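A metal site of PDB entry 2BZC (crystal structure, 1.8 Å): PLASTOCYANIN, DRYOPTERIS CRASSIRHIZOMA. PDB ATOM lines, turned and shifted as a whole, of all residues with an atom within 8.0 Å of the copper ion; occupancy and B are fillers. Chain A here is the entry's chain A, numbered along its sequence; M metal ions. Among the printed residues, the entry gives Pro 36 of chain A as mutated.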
ATOM      1  N   VAL A   5      21.372 -21.466  -3.854  1.00  0.00           N
ATOM      2  CA  VAL A   5      20.317 -22.465  -3.778  1.00  0.00           C
ATOM      3  C   VAL A   5      20.505 -23.435  -4.944  1.00  0.00           C
ATOM      4  O   VAL A   5      20.292 -23.081  -6.113  1.00  0.00           O
ATOM      5  CB  VAL A   5      18.919 -21.797  -3.805  1.00  0.00           C
ATOM      6  CG1 VAL A   5      17.834 -22.818  -3.583  1.00  0.00           C
ATOM      7  CG2 VAL A   5      18.800 -20.672  -2.748  1.00  0.00           C
ATOM      8  N   GLY A   6      20.957 -24.646  -4.617  1.00  0.00           N
ATOM      9  CA  GLY A   6      21.264 -25.678  -5.627  1.00  0.00           C
ATOM     10  C   GLY A   6      22.665 -25.525  -6.226  1.00  0.00           C
ATOM     11  O   GLY A   6      23.462 -24.691  -5.792  1.00  0.00           O
ATOM     12  N   ASN A  11      22.499 -31.257  -7.212  1.00  0.00           N
ATOM     13  CA  ASN A  11      22.354 -31.601  -5.791  1.00  0.00           C
ATOM     14  C   ASN A  11      21.294 -30.736  -5.105  1.00  0.00           C
ATOM     15  O   ASN A  11      21.175 -29.544  -5.411  1.00  0.00           O
ATOM     16  CB  ASN A  11      23.691 -31.444  -5.046  1.00  0.00           C
ATOM     17  CG  ASN A  11      24.749 -32.414  -5.549  1.00  0.00           C
ATOM     18  OD1 ASN A  11      24.560 -33.628  -5.501  1.00  0.00           O
ATOM     19  ND2 ASN A  11      25.865 -31.875  -6.018  1.00  0.00           N
ATOM     20  N   PHE A  12      20.566 -31.325  -4.162  1.00  0.00           N
ATOM     21  CA  PHE A  12      19.519 -30.583  -3.461  1.00  0.00           C
ATOM     22  C   PHE A  12      20.079 -30.039  -2.151  1.00  0.00           C
ATOM     23  O   PHE A  12      19.846 -30.611  -1.066  1.00  0.00           O
ATOM     24  CB  PHE A  12      18.313 -31.473  -3.151  1.00  0.00           C
ATOM     25  CG  PHE A  12      17.817 -32.311  -4.309  1.00  0.00           C
ATOM     26  CD1 PHE A  12      17.764 -31.816  -5.609  1.00  0.00           C
ATOM     27  CD2 PHE A  12      17.358 -33.610  -4.062  1.00  0.00           C
ATOM     28  CE1 PHE A  12      17.279 -32.660  -6.669  1.00  0.00           C
ATOM     29  CE2 PHE A  12      16.868 -34.427  -5.098  1.00  0.00           C
ATOM     30  CZ  PHE A  12      16.843 -33.932  -6.399  1.00  0.00           C
ATOM     31  N   LYS A  13      20.809 -28.943  -2.275  1.00  0.00           N
ATOM     32  CA  LYS A  13      21.594 -28.371  -1.175  1.00  0.00           C
ATOM     33  C   LYS A  13      21.618 -26.875  -1.250  1.00  0.00           C
ATOM     34  O   LYS A  13      21.540 -26.289  -2.345  1.00  0.00           O
ATOM     35  CB  LYS A  13      23.062 -28.842  -1.251  1.00  0.00           C
ATOM     36  CG  LYS A  13      23.280 -30.259  -0.849  1.00  0.00           C
ATOM     37  CD  LYS A  13      24.781 -30.617  -0.867  1.00  0.00           C
ATOM     38  CE  LYS A  13      25.033 -31.855  -0.059  1.00  0.00           C
ATOM     39  NZ  LYS A  13      24.559 -31.570   1.331  1.00  0.00           N
ATOM     40  N   PHE A  14      21.721 -26.238  -0.080  1.00  0.00           N
ATOM     41  CA  PHE A  14      21.977 -24.807  -0.004  1.00  0.00           C
ATOM     42  C   PHE A  14      23.478 -24.644   0.266  1.00  0.00           C
ATOM     43  O   PHE A  14      24.065 -25.464   0.953  1.00  0.00           O
ATOM     44  CB  PHE A  14      21.238 -24.215   1.200  1.00  0.00           C
ATOM     45  CG  PHE A  14      19.753 -24.139   1.015  1.00  0.00           C
ATOM     46  CD1 PHE A  14      19.184 -23.074   0.332  1.00  0.00           C
ATOM     47  CD2 PHE A  14      18.914 -25.126   1.533  1.00  0.00           C
ATOM     48  CE1 PHE A  14      17.762 -22.987   0.162  1.00  0.00           C
ATOM     49  CE2 PHE A  14      17.514 -25.035   1.368  1.00  0.00           C
ATOM     50  CZ  PHE A  14      16.952 -23.974   0.679  1.00  0.00           C
ATOM     51  N   LEU A  31      19.313 -18.725  -7.031  1.00  0.00           N
ATOM     52  CA  LEU A  31      19.403 -20.020  -7.696  1.00  0.00           C
ATOM     53  C   LEU A  31      20.720 -20.231  -8.438  1.00  0.00           C
ATOM     54  O   LEU A  31      21.218 -19.329  -9.094  1.00  0.00           O
ATOM     55  CB  LEU A  31      18.226 -20.208  -8.668  1.00  0.00           C
ATOM     56  CG  LEU A  31      18.035 -21.598  -9.254  1.00  0.00           C
ATOM     57  CD1 LEU A  31      17.541 -22.492  -8.159  1.00  0.00           C
ATOM     58  CD2 LEU A  31      17.066 -21.582 -10.427  1.00  0.00           C
ATOM     59  N   THR A  35      17.905 -26.849 -11.954  1.00  0.00           N
ATOM     60  CA  THR A  35      16.864 -27.398 -11.055  1.00  0.00           C
ATOM     61  C   THR A  35      16.189 -26.270 -10.236  1.00  0.00           C
ATOM     62  O   THR A  35      16.918 -25.550  -9.541  1.00  0.00           O
ATOM     63  CB  THR A  35      17.487 -28.454 -10.091  1.00  0.00           C
ATOM     64  OG1 THR A  35      18.087 -29.479 -10.882  1.00  0.00           O
ATOM     65  CG2 THR A  35      16.404 -29.068  -9.162  1.00  0.00           C
ATOM     66  N   PRO A  36      14.843 -26.104 -10.344  1.00  0.00           N
ATOM     67  CA  PRO A  36      14.110 -25.089  -9.530  1.00  0.00           C
ATOM     68  C   PRO A  36      14.108 -25.460  -8.063  1.00  0.00           C
ATOM     69  O   PRO A  36      14.080 -26.646  -7.728  1.00  0.00           O
ATOM     70  CB  PRO A  36      12.684 -25.116 -10.101  1.00  0.00           C
ATOM     71  CG  PRO A  36      12.779 -25.898 -11.380  1.00  0.00           C
ATOM     72  CD  PRO A  36      13.922 -26.842 -11.222  1.00  0.00           C
ATOM     73  N   HIS A  37      14.113 -24.443  -7.205  1.00  0.00           N
ATOM     74  CA  HIS A  37      14.143 -24.610  -5.759  1.00  0.00           C
ATOM     75  C   HIS A  37      13.345 -23.459  -5.189  1.00  0.00           C
ATOM     76  O   HIS A  37      13.087 -22.473  -5.869  1.00  0.00           O
ATOM     77  CB  HIS A  37      15.589 -24.537  -5.229  1.00  0.00           C
ATOM     78  CG  HIS A  37      16.471 -25.681  -5.664  1.00  0.00           C
ATOM     79  ND1 HIS A  37      16.258 -26.987  -5.271  1.00  0.00           N
ATOM     80  CD2 HIS A  37      17.569 -25.711  -6.456  1.00  0.00           C
ATOM     81  CE1 HIS A  37      17.170 -27.762  -5.804  1.00  0.00           C
ATOM     82  NE2 HIS A  37      17.981 -27.008  -6.539  1.00  0.00           N
ATOM     83  N   ASN A  38      12.994 -23.554  -3.916  1.00  0.00           N
ATOM     84  CA  ASN A  38      12.521 -22.374  -3.202  1.00  0.00           C
ATOM     85  C   ASN A  38      13.084 -22.359  -1.780  1.00  0.00           C
ATOM     86  O   ASN A  38      13.960 -23.191  -1.452  1.00  0.00           O
ATOM     87  CB  ASN A  38      10.991 -22.229  -3.303  1.00  0.00           C
ATOM     88  CG  ASN A  38      10.230 -23.096  -2.323  1.00  0.00           C
ATOM     89  OD1 ASN A  38      10.789 -23.948  -1.630  1.00  0.00           O
ATOM     90  ND2 ASN A  38       8.928 -22.864  -2.247  1.00  0.00           N
ATOM     91  N   ILE A  39      12.640 -21.419  -0.957  1.00  0.00           N
ATOM     92  CA  ILE A  39      13.074 -21.384   0.424  1.00  0.00           C
ATOM     93  C   ILE A  39      11.922 -20.942   1.290  1.00  0.00           C
ATOM     94  O   ILE A  39      11.262 -19.961   1.002  1.00  0.00           O
ATOM     95  CB  ILE A  39      14.349 -20.533   0.590  1.00  0.00           C
ATOM     96  CG1 ILE A  39      14.857 -20.518   2.066  1.00  0.00           C
ATOM     97  CG2 ILE A  39      14.211 -19.109  -0.104  1.00  0.00           C
ATOM     98  CD1 ILE A  39      14.318 -19.372   2.892  1.00  0.00           C
ATOM     99  N   LEU A  65       8.598 -20.942  -7.211  1.00  0.00           N
ATOM    100  CA  LEU A  65       9.955 -21.479  -7.366  1.00  0.00           C
ATOM    101  C   LEU A  65      10.885 -20.432  -7.921  1.00  0.00           C
ATOM    102  O   LEU A  65      10.470 -19.584  -8.713  1.00  0.00           O
ATOM    103  CB  LEU A  65       9.937 -22.727  -8.262  1.00  0.00           C
ATOM    104  CG  LEU A  65       9.196 -23.929  -7.706  1.00  0.00           C
ATOM    105  CD1 LEU A  65       8.990 -25.023  -8.766  1.00  0.00           C
ATOM    106  CD2 LEU A  65       9.861 -24.488  -6.474  1.00  0.00           C
ATOM    107  N   TYR A  86      13.907 -24.604   4.608  1.00  0.00           N
ATOM    108  CA  TYR A  86      13.955 -25.769   3.727  1.00  0.00           C
ATOM    109  C   TYR A  86      13.479 -25.382   2.327  1.00  0.00           C
ATOM    110  O   TYR A  86      12.867 -24.321   2.154  1.00  0.00           O
ATOM    111  CB  TYR A  86      13.118 -26.912   4.335  1.00  0.00           C
ATOM    112  CG  TYR A  86      11.665 -26.565   4.478  1.00  0.00           C
ATOM    113  CD1 TYR A  86      10.796 -26.650   3.385  1.00  0.00           C
ATOM    114  CD2 TYR A  86      11.152 -26.093   5.699  1.00  0.00           C
ATOM    115  CE1 TYR A  86       9.428 -26.313   3.530  1.00  0.00           C
ATOM    116  CE2 TYR A  86       9.818 -25.768   5.842  1.00  0.00           C
ATOM    117  CZ  TYR A  86       8.957 -25.874   4.755  1.00  0.00           C
ATOM    118  OH  TYR A  86       7.632 -25.546   4.921  1.00  0.00           O
ATOM    119  N   CYS A  87      13.755 -26.246   1.351  1.00  0.00           N
ATOM    120  CA  CYS A  87      13.169 -26.181   0.030  1.00  0.00           C
ATOM    121  C   CYS A  87      11.911 -27.042  -0.062  1.00  0.00           C
ATOM    122  O   CYS A  87      11.987 -28.233   0.229  1.00  0.00           O
ATOM    123  CB  CYS A  87      14.177 -26.670  -1.045  1.00  0.00           C
ATOM    124  SG  CYS A  87      13.391 -26.758  -2.696  1.00  0.00           S
ATOM    125  N   THR A  88      10.792 -26.453  -0.495  1.00  0.00           N
ATOM    126  CA  THR A  88       9.501 -27.162  -0.594  1.00  0.00           C
ATOM    127  C   THR A  88       9.569 -28.446  -1.454  1.00  0.00           C
ATOM    128  O   THR A  88       9.288 -29.520  -0.950  1.00  0.00           O
ATOM    129  CB  THR A  88       8.338 -26.200  -1.063  1.00  0.00           C
ATOM    130  OG1 THR A  88       8.108 -25.198  -0.063  1.00  0.00           O
ATOM    131  CG2 THR A  88       7.045 -26.959  -1.342  1.00  0.00           C
ATOM    132  N   PRO A  89       9.935 -28.334  -2.739  1.00  0.00           N
ATOM    133  CA  PRO A  89       9.979 -29.619  -3.495  1.00  0.00           C
ATOM    134  C   PRO A  89      10.951 -30.681  -2.973  1.00  0.00           C
ATOM    135  O   PRO A  89      10.597 -31.862  -2.981  1.00  0.00           O
ATOM    136  CB  PRO A  89      10.337 -29.206  -4.923  1.00  0.00           C
ATOM    137  CG  PRO A  89      10.754 -27.799  -4.849  1.00  0.00           C
ATOM    138  CD  PRO A  89      10.209 -27.175  -3.617  1.00  0.00           C
ATOM    139  N   HIS A  90      12.140 -30.271  -2.494  1.00  0.00           N
ATOM    140  CA  HIS A  90      13.169 -31.226  -2.030  1.00  0.00           C
ATOM    141  C   HIS A  90      13.272 -31.396  -0.500  1.00  0.00           C
ATOM    142  O   HIS A  90      14.245 -31.963  -0.015  1.00  0.00           O
ATOM    143  CB  HIS A  90      14.514 -30.933  -2.653  1.00  0.00           C
ATOM    144  CG  HIS A  90      14.466 -30.887  -4.152  1.00  0.00           C
ATOM    145  ND1 HIS A  90      14.528 -29.699  -4.860  1.00  0.00           N
ATOM    146  CD2 HIS A  90      14.261 -31.850  -5.070  1.00  0.00           C
ATOM    147  CE1 HIS A  90      14.413 -29.942  -6.143  1.00  0.00           C
ATOM    148  NE2 HIS A  90      14.255 -31.251  -6.307  1.00  0.00           N
ATOM    149  N   LYS A  91      12.234 -30.998   0.210  1.00  0.00           N
ATOM    150  CA  LYS A  91      12.167 -31.066   1.679  1.00  0.00           C
ATOM    151  C   LYS A  91      12.511 -32.459   2.204  1.00  0.00           C
ATOM    152  O   LYS A  91      13.332 -32.618   3.114  1.00  0.00           O
ATOM    153  CB  LYS A  91      10.808 -30.634   2.178  1.00  0.00           C
ATOM    154  CG  LYS A  91      10.761 -30.424   3.664  1.00  0.00           C
ATOM    155  CD  LYS A  91       9.357 -30.039   4.112  1.00  0.00           C
ATOM    156  CE  LYS A  91       9.399 -29.380   5.493  1.00  0.00           C
ATOM    157  NZ  LYS A  91       9.870 -30.360   6.500  1.00  0.00           N
ATOM    158  N   ALA A  93      14.188 -34.641   0.599  1.00  0.00           N
ATOM    159  CA  ALA A  93      15.544 -34.956   0.166  1.00  0.00           C
ATOM    160  C   ALA A  93      16.564 -34.212   1.034  1.00  0.00           C
ATOM    161  O   ALA A  93      17.747 -34.133   0.686  1.00  0.00           O
ATOM    162  CB  ALA A  93      15.722 -34.608  -1.303  1.00  0.00           C
ATOM    163  N   MET A  95      16.941 -31.108   1.936  1.00  0.00           N
ATOM    164  CA  MET A  95      17.423 -29.833   1.421  1.00  0.00           C
ATOM    165  C   MET A  95      17.032 -28.733   2.407  1.00  0.00           C
ATOM    166  O   MET A  95      15.921 -28.172   2.343  1.00  0.00           O
ATOM    167  CB  MET A  95      16.867 -29.538   0.028  1.00  0.00           C
ATOM    168  CG  MET A  95      17.432 -28.239  -0.559  1.00  0.00           C
ATOM    169  SD  MET A  95      17.256 -28.043  -2.316  1.00  0.00           S
ATOM    170  CE  MET A  95      17.915 -26.353  -2.507  1.00  0.00           C
ATOM    171  N   LYS A  96      17.960 -28.421   3.316  1.00  0.00           N
ATOM    172  CA  LYS A  96      17.634 -27.542   4.440  1.00  0.00           C
ATOM    173  C   LYS A  96      18.855 -26.806   4.883  1.00  0.00           C
ATOM    174  O   LYS A  96      19.986 -27.175   4.499  1.00  0.00           O
ATOM    175  CB  LYS A  96      17.005 -28.337   5.629  1.00  0.00           C
ATOM    176  CG  LYS A  96      17.791 -29.459   6.297  1.00  0.00           C
ATOM    177  CD  LYS A  96      16.774 -30.487   6.775  1.00  0.00           C
ATOM    178  CE  LYS A  96      17.090 -31.124   8.165  1.00  0.00           C
ATOM    179  NZ  LYS A  96      16.593 -30.175   9.251  1.00  0.00           N
HETATM  180 CU    CU M   1      14.889 -27.766  -4.010  1.00  0.00          CU
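ND1 of His 37 binds the copper ion.
ND1 of His 90 is bound to the copper ion (2.1 Å).
The copper ion is bound by SG of Cys 87, at 2.2 Å.
The copper ion has three donor atoms within binding distance.
Slightly farther from the copper ion lies the side-chain sulfur (SD) of Met 95 (2.9 Å).
N of Cys 87 sits at hydrogen-bond distance from O of Met 95, at 3.1 Å.
SD of Met 95 lies close to ND1 of His 37 (3.3 Å).
O of His 90 sits at hydrogen-bond distance from N of Met 95 (3.4 Å).
SG of Cys 87 sits close to N of Asn 38 (3.5 Å).
The side-chain sulfur (SD) of Met 95 is in hydrogen-bond range of the backbone NH (N) of Lys 13 (3.7 Å).
Residues that only touch the copper ion: Pro 36.
The nearest printed residue that does not touch the copper ion is Pro 89 (4.2 Å).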
